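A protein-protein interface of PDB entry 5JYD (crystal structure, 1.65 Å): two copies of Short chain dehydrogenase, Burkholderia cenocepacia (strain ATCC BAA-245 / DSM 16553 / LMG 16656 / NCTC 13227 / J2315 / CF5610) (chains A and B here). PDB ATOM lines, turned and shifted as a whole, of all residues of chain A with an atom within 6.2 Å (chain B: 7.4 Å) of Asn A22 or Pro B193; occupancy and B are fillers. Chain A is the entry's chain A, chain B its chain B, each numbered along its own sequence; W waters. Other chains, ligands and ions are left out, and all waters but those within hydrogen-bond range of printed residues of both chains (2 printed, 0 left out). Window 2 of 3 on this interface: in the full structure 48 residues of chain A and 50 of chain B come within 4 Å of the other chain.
Hydrophobic or aromatic side chains of chain A that line the printed part of chain B: Leu A20, Pro A23 and Val A24. Hydrophobic or aromatic side chains of chain B within 4 Å of the printed part of chain A: Pro B192 and Pro B193. Along chain B the printed residues that touch a printed residue of chain A span positions 146 to 294. Among the printed residues, no Asp or Glu carboxylate lies within 4 Å of a Lys or Arg side-chain nitrogen of the other chain.
No position is printed for both chains. Of the 12 pairs that touch across the chains among the printed residues, none has its exchanged pair printed and touching as well.
N of Ser B196 lies within hydrogen-bond range of O of Asp B146 (3.1 Å). OD1 of Asn A22 is in hydrogen-bond range of N of Val A24, at 2.9 Å. The backbone NH (N) of Gly B194 sits at hydrogen-bond distance from the backbone carbonyl oxygen (O) of Gly B237 (2.8 Å).
Printed residues of chain B within 4 Å of Thr A21: Gly B194 (3.2 Å). Asn A22 touches two residues of chain B. Printed residues of chain B within 4 Å of Val A24: Gly B234, Pro B235 and Gly B237. Pro B193 touches two residues of chain A. Printed residues of chain A within 4 Å of Gly B234: Val A24. The nearest residue of chain B that does not touch Asn A22 is Arg B236 (4.04 Å). The nearest residue of chain A that does not touch Pro B193 is Thr A21 (4.3 Å).
Water W1 bridges the backbone carbonyl oxygen (O) of Pro B235 (2.8 Å) and the side-chain amide nitrogen (ND2) of Asn A22 (2.9 Å). Water W2 bridges O of Gly B194 (2.9 Å) and N of Thr A21 (3.3 Å).
Among the printed residues, merely in contact across the chains: Leu A20 with Asp B146 (3.9 Å), Leu A20 with Pro B192 (3.4 Å), Leu A20 with Pro B193 (3.9 Å), Leu A20 with Gly B194 (3.7 Å), Thr A21 with Gly B194 (3.2 Å), Asn A22 with Pro B193 (3.6 Å), Asn A22 with Gly B237 (3.3 Å), Pro A23 with Gly B237 (3.4 Å), Pro A23 with Ser B294 (3.5 Å), Val A24 with Gly B234 (3.1 Å), Val A24 with Pro B235 (3.7 Å) and Val A24 with Gly B237 (3.9 Å).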
ATOM      1  N   LEU A  20     -22.191 -12.609  22.464  1.00  0.00           N
ATOM      2  CA  LEU A  20     -21.889 -13.729  21.566  1.00  0.00           C
ATOM      3  C   LEU A  20     -23.147 -14.499  21.179  1.00  0.00           C
ATOM      4  O   LEU A  20     -23.930 -14.868  22.039  1.00  0.00           O
ATOM      5  CB  LEU A  20     -20.892 -14.696  22.223  1.00  0.00           C
ATOM      6  CG  LEU A  20     -19.488 -14.162  22.510  1.00  0.00           C
ATOM      7  CD1 LEU A  20     -18.612 -15.282  23.013  1.00  0.00           C
ATOM      8  CD2 LEU A  20     -18.880 -13.529  21.281  1.00  0.00           C
ATOM      9  N   THR A  21     -23.319 -14.763  19.883  1.00  0.00           N
ATOM     10  CA  THR A  21     -24.408 -15.602  19.395  1.00  0.00           C
ATOM     11  C   THR A  21     -23.851 -16.667  18.465  1.00  0.00           C
ATOM     12  O   THR A  21     -22.970 -16.375  17.653  1.00  0.00           O
ATOM     13  CB  THR A  21     -25.441 -14.785  18.635  1.00  0.00           C
ATOM     14  OG1 THR A  21     -24.828 -14.239  17.454  1.00  0.00           O
ATOM     15  CG2 THR A  21     -25.994 -13.642  19.496  1.00  0.00           C
ATOM     16  N   ASN A  22     -24.369 -17.889  18.573  1.00  0.00           N
ATOM     17  CA  ASN A  22     -24.007 -18.944  17.609  1.00  0.00           C
ATOM     18  C   ASN A  22     -24.601 -18.601  16.243  1.00  0.00           C
ATOM     19  O   ASN A  22     -25.835 -18.612  16.100  1.00  0.00           O
ATOM     20  CB  ASN A  22     -24.520 -20.306  18.050  1.00  0.00           C
ATOM     21  CG  ASN A  22     -23.985 -21.441  17.194  1.00  0.00           C
ATOM     22  OD1 ASN A  22     -23.669 -21.258  16.003  1.00  0.00           O
ATOM     23  ND2 ASN A  22     -23.880 -22.625  17.798  1.00  0.00           N
ATOM     24  N   PRO A  23     -23.789 -18.330  15.211  1.00  0.00           N
ATOM     25  CA  PRO A  23     -24.367 -17.966  13.900  1.00  0.00           C
ATOM     26  C   PRO A  23     -25.134 -19.091  13.223  1.00  0.00           C
ATOM     27  O   PRO A  23     -26.038 -18.801  12.427  1.00  0.00           O
ATOM     28  CB  PRO A  23     -23.139 -17.522  13.078  1.00  0.00           C
ATOM     29  CG  PRO A  23     -21.972 -18.092  13.748  1.00  0.00           C
ATOM     30  CD  PRO A  23     -22.317 -18.390  15.179  1.00  0.00           C
ATOM     31  N   VAL A  24     -24.835 -20.355  13.530  1.00  0.00           N
ATOM     32  CA  VAL A  24     -25.442 -21.477  12.815  1.00  0.00           C
ATOM     33  C   VAL A  24     -26.963 -21.408  12.886  1.00  0.00           C
ATOM     34  O   VAL A  24     -27.654 -21.541  11.874  1.00  0.00           O
ATOM     35  CB  VAL A  24     -24.923 -22.818  13.369  1.00  0.00           C
ATOM     36  CG1 VAL A  24     -25.731 -24.002  12.812  1.00  0.00           C
ATOM     37  CG2 VAL A  24     -23.448 -23.007  13.037  1.00  0.00           C
ATOM     38  N   ASP A  25     -27.512 -21.247  14.088  1.00  0.00           N
ATOM     39  CA  ASP A  25     -28.954 -21.346  14.282  1.00  0.00           C
ATOM     40  C   ASP A  25     -29.606 -19.983  14.484  1.00  0.00           C
ATOM     41  O   ASP A  25     -30.727 -19.902  14.994  1.00  0.00           O
ATOM     42  CB  ASP A  25     -29.251 -22.268  15.461  1.00  0.00           C
ATOM     43  CG  ASP A  25     -28.315 -22.032  16.605  1.00  0.00           C
ATOM     44  OD1 ASP A  25     -28.356 -20.916  17.154  1.00  0.00           O
ATOM     45  OD2 ASP A  25     -27.524 -22.942  16.939  1.00  0.00           O
ATOM     46  N   LEU A  26     -28.928 -18.920  14.079  1.00  0.00           N
ATOM     47  CA  LEU A  26     -29.471 -17.570  14.151  1.00  0.00           C
ATOM     48  C   LEU A  26     -30.602 -17.353  13.151  1.00  0.00           C
ATOM     49  O   LEU A  26     -31.417 -16.441  13.343  1.00  0.00           O
ATOM     50  CB  LEU A  26     -28.337 -16.574  13.898  1.00  0.00           C
ATOM     51  CG  LEU A  26     -28.392 -15.135  14.388  1.00  0.00           C
ATOM     52  CD1 LEU A  26     -28.666 -15.082  15.888  1.00  0.00           C
ATOM     53  CD2 LEU A  26     -27.064 -14.449  14.058  1.00  0.00           C
ATOM     54  N   ASP B 146     -12.380 -15.341  23.143  1.00  0.00           N
ATOM     55  CA  ASP B 146     -13.328 -15.487  22.044  1.00  0.00           C
ATOM     56  C   ASP B 146     -12.936 -14.710  20.785  1.00  0.00           C
ATOM     57  O   ASP B 146     -13.711 -14.712  19.822  1.00  0.00           O
ATOM     58  CB  ASP B 146     -14.746 -15.086  22.524  1.00  0.00           C
ATOM     59  CG  ASP B 146     -14.770 -13.741  23.237  1.00  0.00           C
ATOM     60  OD1 ASP B 146     -15.199 -13.690  24.401  1.00  0.00           O
ATOM     61  OD2 ASP B 146     -14.361 -12.742  22.622  1.00  0.00           O
ATOM     62  N   HIS B 190     -11.327 -23.261  24.393  1.00  0.00           N
ATOM     63  CA  HIS B 190     -11.773 -22.071  25.104  1.00  0.00           C
ATOM     64  C   HIS B 190     -12.823 -21.270  24.346  1.00  0.00           C
ATOM     65  O   HIS B 190     -13.535 -20.457  24.956  1.00  0.00           O
ATOM     66  CB  HIS B 190     -10.582 -21.148  25.371  1.00  0.00           C
ATOM     67  CG  HIS B 190      -9.520 -21.754  26.234  1.00  0.00           C
ATOM     68  ND1 HIS B 190      -9.532 -21.647  27.605  1.00  0.00           N
ATOM     69  CD2 HIS B 190      -8.406 -22.458  25.917  1.00  0.00           C
ATOM     70  CE1 HIS B 190      -8.481 -22.275  28.101  1.00  0.00           C
ATOM     71  NE2 HIS B 190      -7.774 -22.765  27.095  1.00  0.00           N
ATOM     72  N   LEU B 191     -12.916 -21.455  23.045  1.00  0.00           N
ATOM     73  CA  LEU B 191     -13.731 -20.586  22.218  1.00  0.00           C
ATOM     74  C   LEU B 191     -15.197 -21.008  22.264  1.00  0.00           C
ATOM     75  O   LEU B 191     -15.516 -22.139  21.881  1.00  0.00           O
ATOM     76  CB  LEU B 191     -13.215 -20.616  20.789  1.00  0.00           C
ATOM     77  CG  LEU B 191     -11.750 -20.244  20.587  1.00  0.00           C
ATOM     78  CD1 LEU B 191     -11.431 -20.449  19.142  1.00  0.00           C
ATOM     79  CD2 LEU B 191     -11.524 -18.814  21.025  1.00  0.00           C
ATOM     80  N   PRO B 192     -16.111 -20.149  22.706  1.00  0.00           N
ATOM     81  CA  PRO B 192     -17.516 -20.513  22.706  1.00  0.00           C
ATOM     82  C   PRO B 192     -18.134 -20.263  21.344  1.00  0.00           C
ATOM     83  O   PRO B 192     -17.546 -19.563  20.503  1.00  0.00           O
ATOM     84  CB  PRO B 192     -18.119 -19.579  23.766  1.00  0.00           C
ATOM     85  CG  PRO B 192     -17.285 -18.365  23.660  1.00  0.00           C
ATOM     86  CD  PRO B 192     -15.898 -18.823  23.318  1.00  0.00           C
ATOM     87  N   PRO B 193     -19.318 -20.799  21.088  1.00  0.00           N
ATOM     88  CA  PRO B 193     -20.032 -20.428  19.863  1.00  0.00           C
ATOM     89  C   PRO B 193     -20.187 -18.913  19.796  1.00  0.00           C
ATOM     90  O   PRO B 193     -20.435 -18.254  20.813  1.00  0.00           O
ATOM     91  CB  PRO B 193     -21.383 -21.145  20.007  1.00  0.00           C
ATOM     92  CG  PRO B 193     -21.140 -22.212  21.007  1.00  0.00           C
ATOM     93  CD  PRO B 193     -20.150 -21.644  21.965  1.00  0.00           C
ATOM     94  N   GLY B 194     -19.985 -18.361  18.588  1.00  0.00           N
ATOM     95  CA  GLY B 194     -19.898 -16.926  18.379  1.00  0.00           C
ATOM     96  C   GLY B 194     -18.486 -16.370  18.329  1.00  0.00           C
ATOM     97  O   GLY B 194     -18.319 -15.192  17.991  1.00  0.00           O
ATOM     98  N   ALA B 195     -17.474 -17.167  18.670  1.00  0.00           N
ATOM     99  CA  ALA B 195     -16.087 -16.708  18.657  1.00  0.00           C
ATOM    100  C   ALA B 195     -15.558 -16.581  17.216  1.00  0.00           C
ATOM    101  O   ALA B 195     -16.157 -17.080  16.254  1.00  0.00           O
ATOM    102  CB  ALA B 195     -15.214 -17.662  19.465  1.00  0.00           C
ATOM    103  N   SER B 196     -14.389 -15.926  17.082  1.00  0.00           N
ATOM    104  CA  SER B 196     -13.709 -15.735  15.806  1.00  0.00           C
ATOM    105  C   SER B 196     -12.230 -16.068  15.913  1.00  0.00           C
ATOM    106  O   SER B 196     -11.602 -15.803  16.937  1.00  0.00           O
ATOM    107  CB  SER B 196     -13.819 -14.289  15.320  1.00  0.00           C
ATOM    108  OG  SER B 196     -14.855 -14.146  14.402  1.00  0.00           O
ATOM    109  N   LEU B 233     -14.962 -25.895  11.965  1.00  0.00           N
ATOM    110  CA  LEU B 233     -15.481 -25.195  13.142  1.00  0.00           C
ATOM    111  C   LEU B 233     -16.758 -24.405  12.887  1.00  0.00           C
ATOM    112  O   LEU B 233     -17.502 -24.133  13.842  1.00  0.00           O
ATOM    113  CB  LEU B 233     -14.418 -24.243  13.705  1.00  0.00           C
ATOM    114  CG  LEU B 233     -13.117 -24.888  14.164  1.00  0.00           C
ATOM    115  CD1 LEU B 233     -12.208 -23.781  14.682  1.00  0.00           C
ATOM    116  CD2 LEU B 233     -13.350 -25.981  15.219  1.00  0.00           C
ATOM    117  N   GLY B 234     -17.033 -24.045  11.635  1.00  0.00           N
ATOM    118  CA  GLY B 234     -18.250 -23.346  11.289  1.00  0.00           C
ATOM    119  C   GLY B 234     -19.501 -24.020  11.809  1.00  0.00           C
ATOM    120  O   GLY B 234     -20.393 -23.372  12.365  1.00  0.00           O
ATOM    121  N   PRO B 235     -19.609 -25.339  11.623  1.00  0.00           N
ATOM    122  CA  PRO B 235     -20.785 -26.062  12.142  1.00  0.00           C
ATOM    123  C   PRO B 235     -20.936 -25.980  13.658  1.00  0.00           C
ATOM    124  O   PRO B 235     -22.035 -26.198  14.184  1.00  0.00           O
ATOM    125  CB  PRO B 235     -20.541 -27.511  11.679  1.00  0.00           C
ATOM    126  CG  PRO B 235     -19.640 -27.394  10.494  1.00  0.00           C
ATOM    127  CD  PRO B 235     -18.743 -26.207  10.806  1.00  0.00           C
ATOM    128  N   ARG B 236     -19.863 -25.666  14.369  1.00  0.00           N
ATOM    129  CA  ARG B 236     -19.900 -25.492  15.808  1.00  0.00           C
ATOM    130  C   ARG B 236     -20.054 -24.034  16.227  1.00  0.00           C
ATOM    131  O   ARG B 236     -20.019 -23.748  17.425  1.00  0.00           O
ATOM    132  CB  ARG B 236     -18.628 -26.052  16.445  1.00  0.00           C
ATOM    133  CG  ARG B 236     -18.293 -27.490  16.077  1.00  0.00           C
ATOM    134  CD  ARG B 236     -16.856 -27.798  16.476  1.00  0.00           C
ATOM    135  NE  ARG B 236     -16.556 -27.282  17.813  1.00  0.00           N
ATOM    136  CZ  ARG B 236     -15.451 -27.555  18.489  1.00  0.00           C
ATOM    137  NH1 ARG B 236     -14.532 -28.353  17.956  1.00  0.00           N
ATOM    138  NH2 ARG B 236     -15.275 -27.032  19.699  1.00  0.00           N
ATOM    139  N   GLY B 237     -20.204 -23.114  15.285  1.00  0.00           N
ATOM    140  CA  GLY B 237     -20.442 -21.730  15.628  1.00  0.00           C
ATOM    141  C   GLY B 237     -19.218 -20.858  15.789  1.00  0.00           C
ATOM    142  O   GLY B 237     -19.352 -19.743  16.286  1.00  0.00           O
ATOM    143  N   ILE B 238     -18.036 -21.320  15.376  1.00  0.00           N
ATOM    144  CA  ILE B 238     -16.804 -20.543  15.408  1.00  0.00           C
ATOM    145  C   ILE B 238     -16.406 -20.220  13.969  1.00  0.00           C
ATOM    146  O   ILE B 238     -16.322 -21.123  13.127  1.00  0.00           O
ATOM    147  CB  ILE B 238     -15.695 -21.327  16.124  1.00  0.00           C
ATOM    148  CG1 ILE B 238     -16.075 -21.600  17.585  1.00  0.00           C
ATOM    149  CG2 ILE B 238     -14.375 -20.564  16.037  1.00  0.00           C
ATOM    150  CD1 ILE B 238     -15.301 -22.769  18.155  1.00  0.00           C
ATOM    151  N   ARG B 239     -16.157 -18.939  13.681  1.00  0.00           N
ATOM    152  CA  ARG B 239     -15.830 -18.490  12.335  1.00  0.00           C
ATOM    153  C   ARG B 239     -14.317 -18.285  12.217  1.00  0.00           C
ATOM    154  O   ARG B 239     -13.669 -17.779  13.139  1.00  0.00           O
ATOM    155  CB  ARG B 239     -16.591 -17.203  11.959  1.00  0.00           C
ATOM    156  CG  ARG B 239     -18.129 -17.404  11.919  1.00  0.00           C
ATOM    157  CD  ARG B 239     -18.934 -16.168  11.458  1.00  0.00           C
ATOM    158  NE  ARG B 239     -18.826 -15.068  12.405  1.00  0.00           N
ATOM    159  CZ  ARG B 239     -18.041 -14.004  12.244  1.00  0.00           C
ATOM    160  NH1 ARG B 239     -17.264 -13.862  11.174  1.00  0.00           N
ATOM    161  NH2 ARG B 239     -18.024 -13.072  13.183  1.00  0.00           N
ATOM    162  N   SER B 294     -22.108 -12.545  10.365  1.00  0.00           N
ATOM    163  CA  SER B 294     -22.285 -13.924  10.809  1.00  0.00           C
ATOM    164  C   SER B 294     -22.235 -14.966   9.689  1.00  0.00           C
ATOM    165  O   SER B 294     -22.241 -16.169   9.989  1.00  0.00           O
ATOM    166  CB  SER B 294     -23.605 -14.045  11.601  1.00  0.00           C
ATOM    167  OG  SER B 294     -24.711 -13.451  10.917  1.00  0.00           O
HETATM  168  O   HOH W   1     -23.467 -25.190  16.410  1.00  0.00           O
HETATM  169  O   HOH W   2     -20.808 -13.709  18.102  1.00  0.00           O
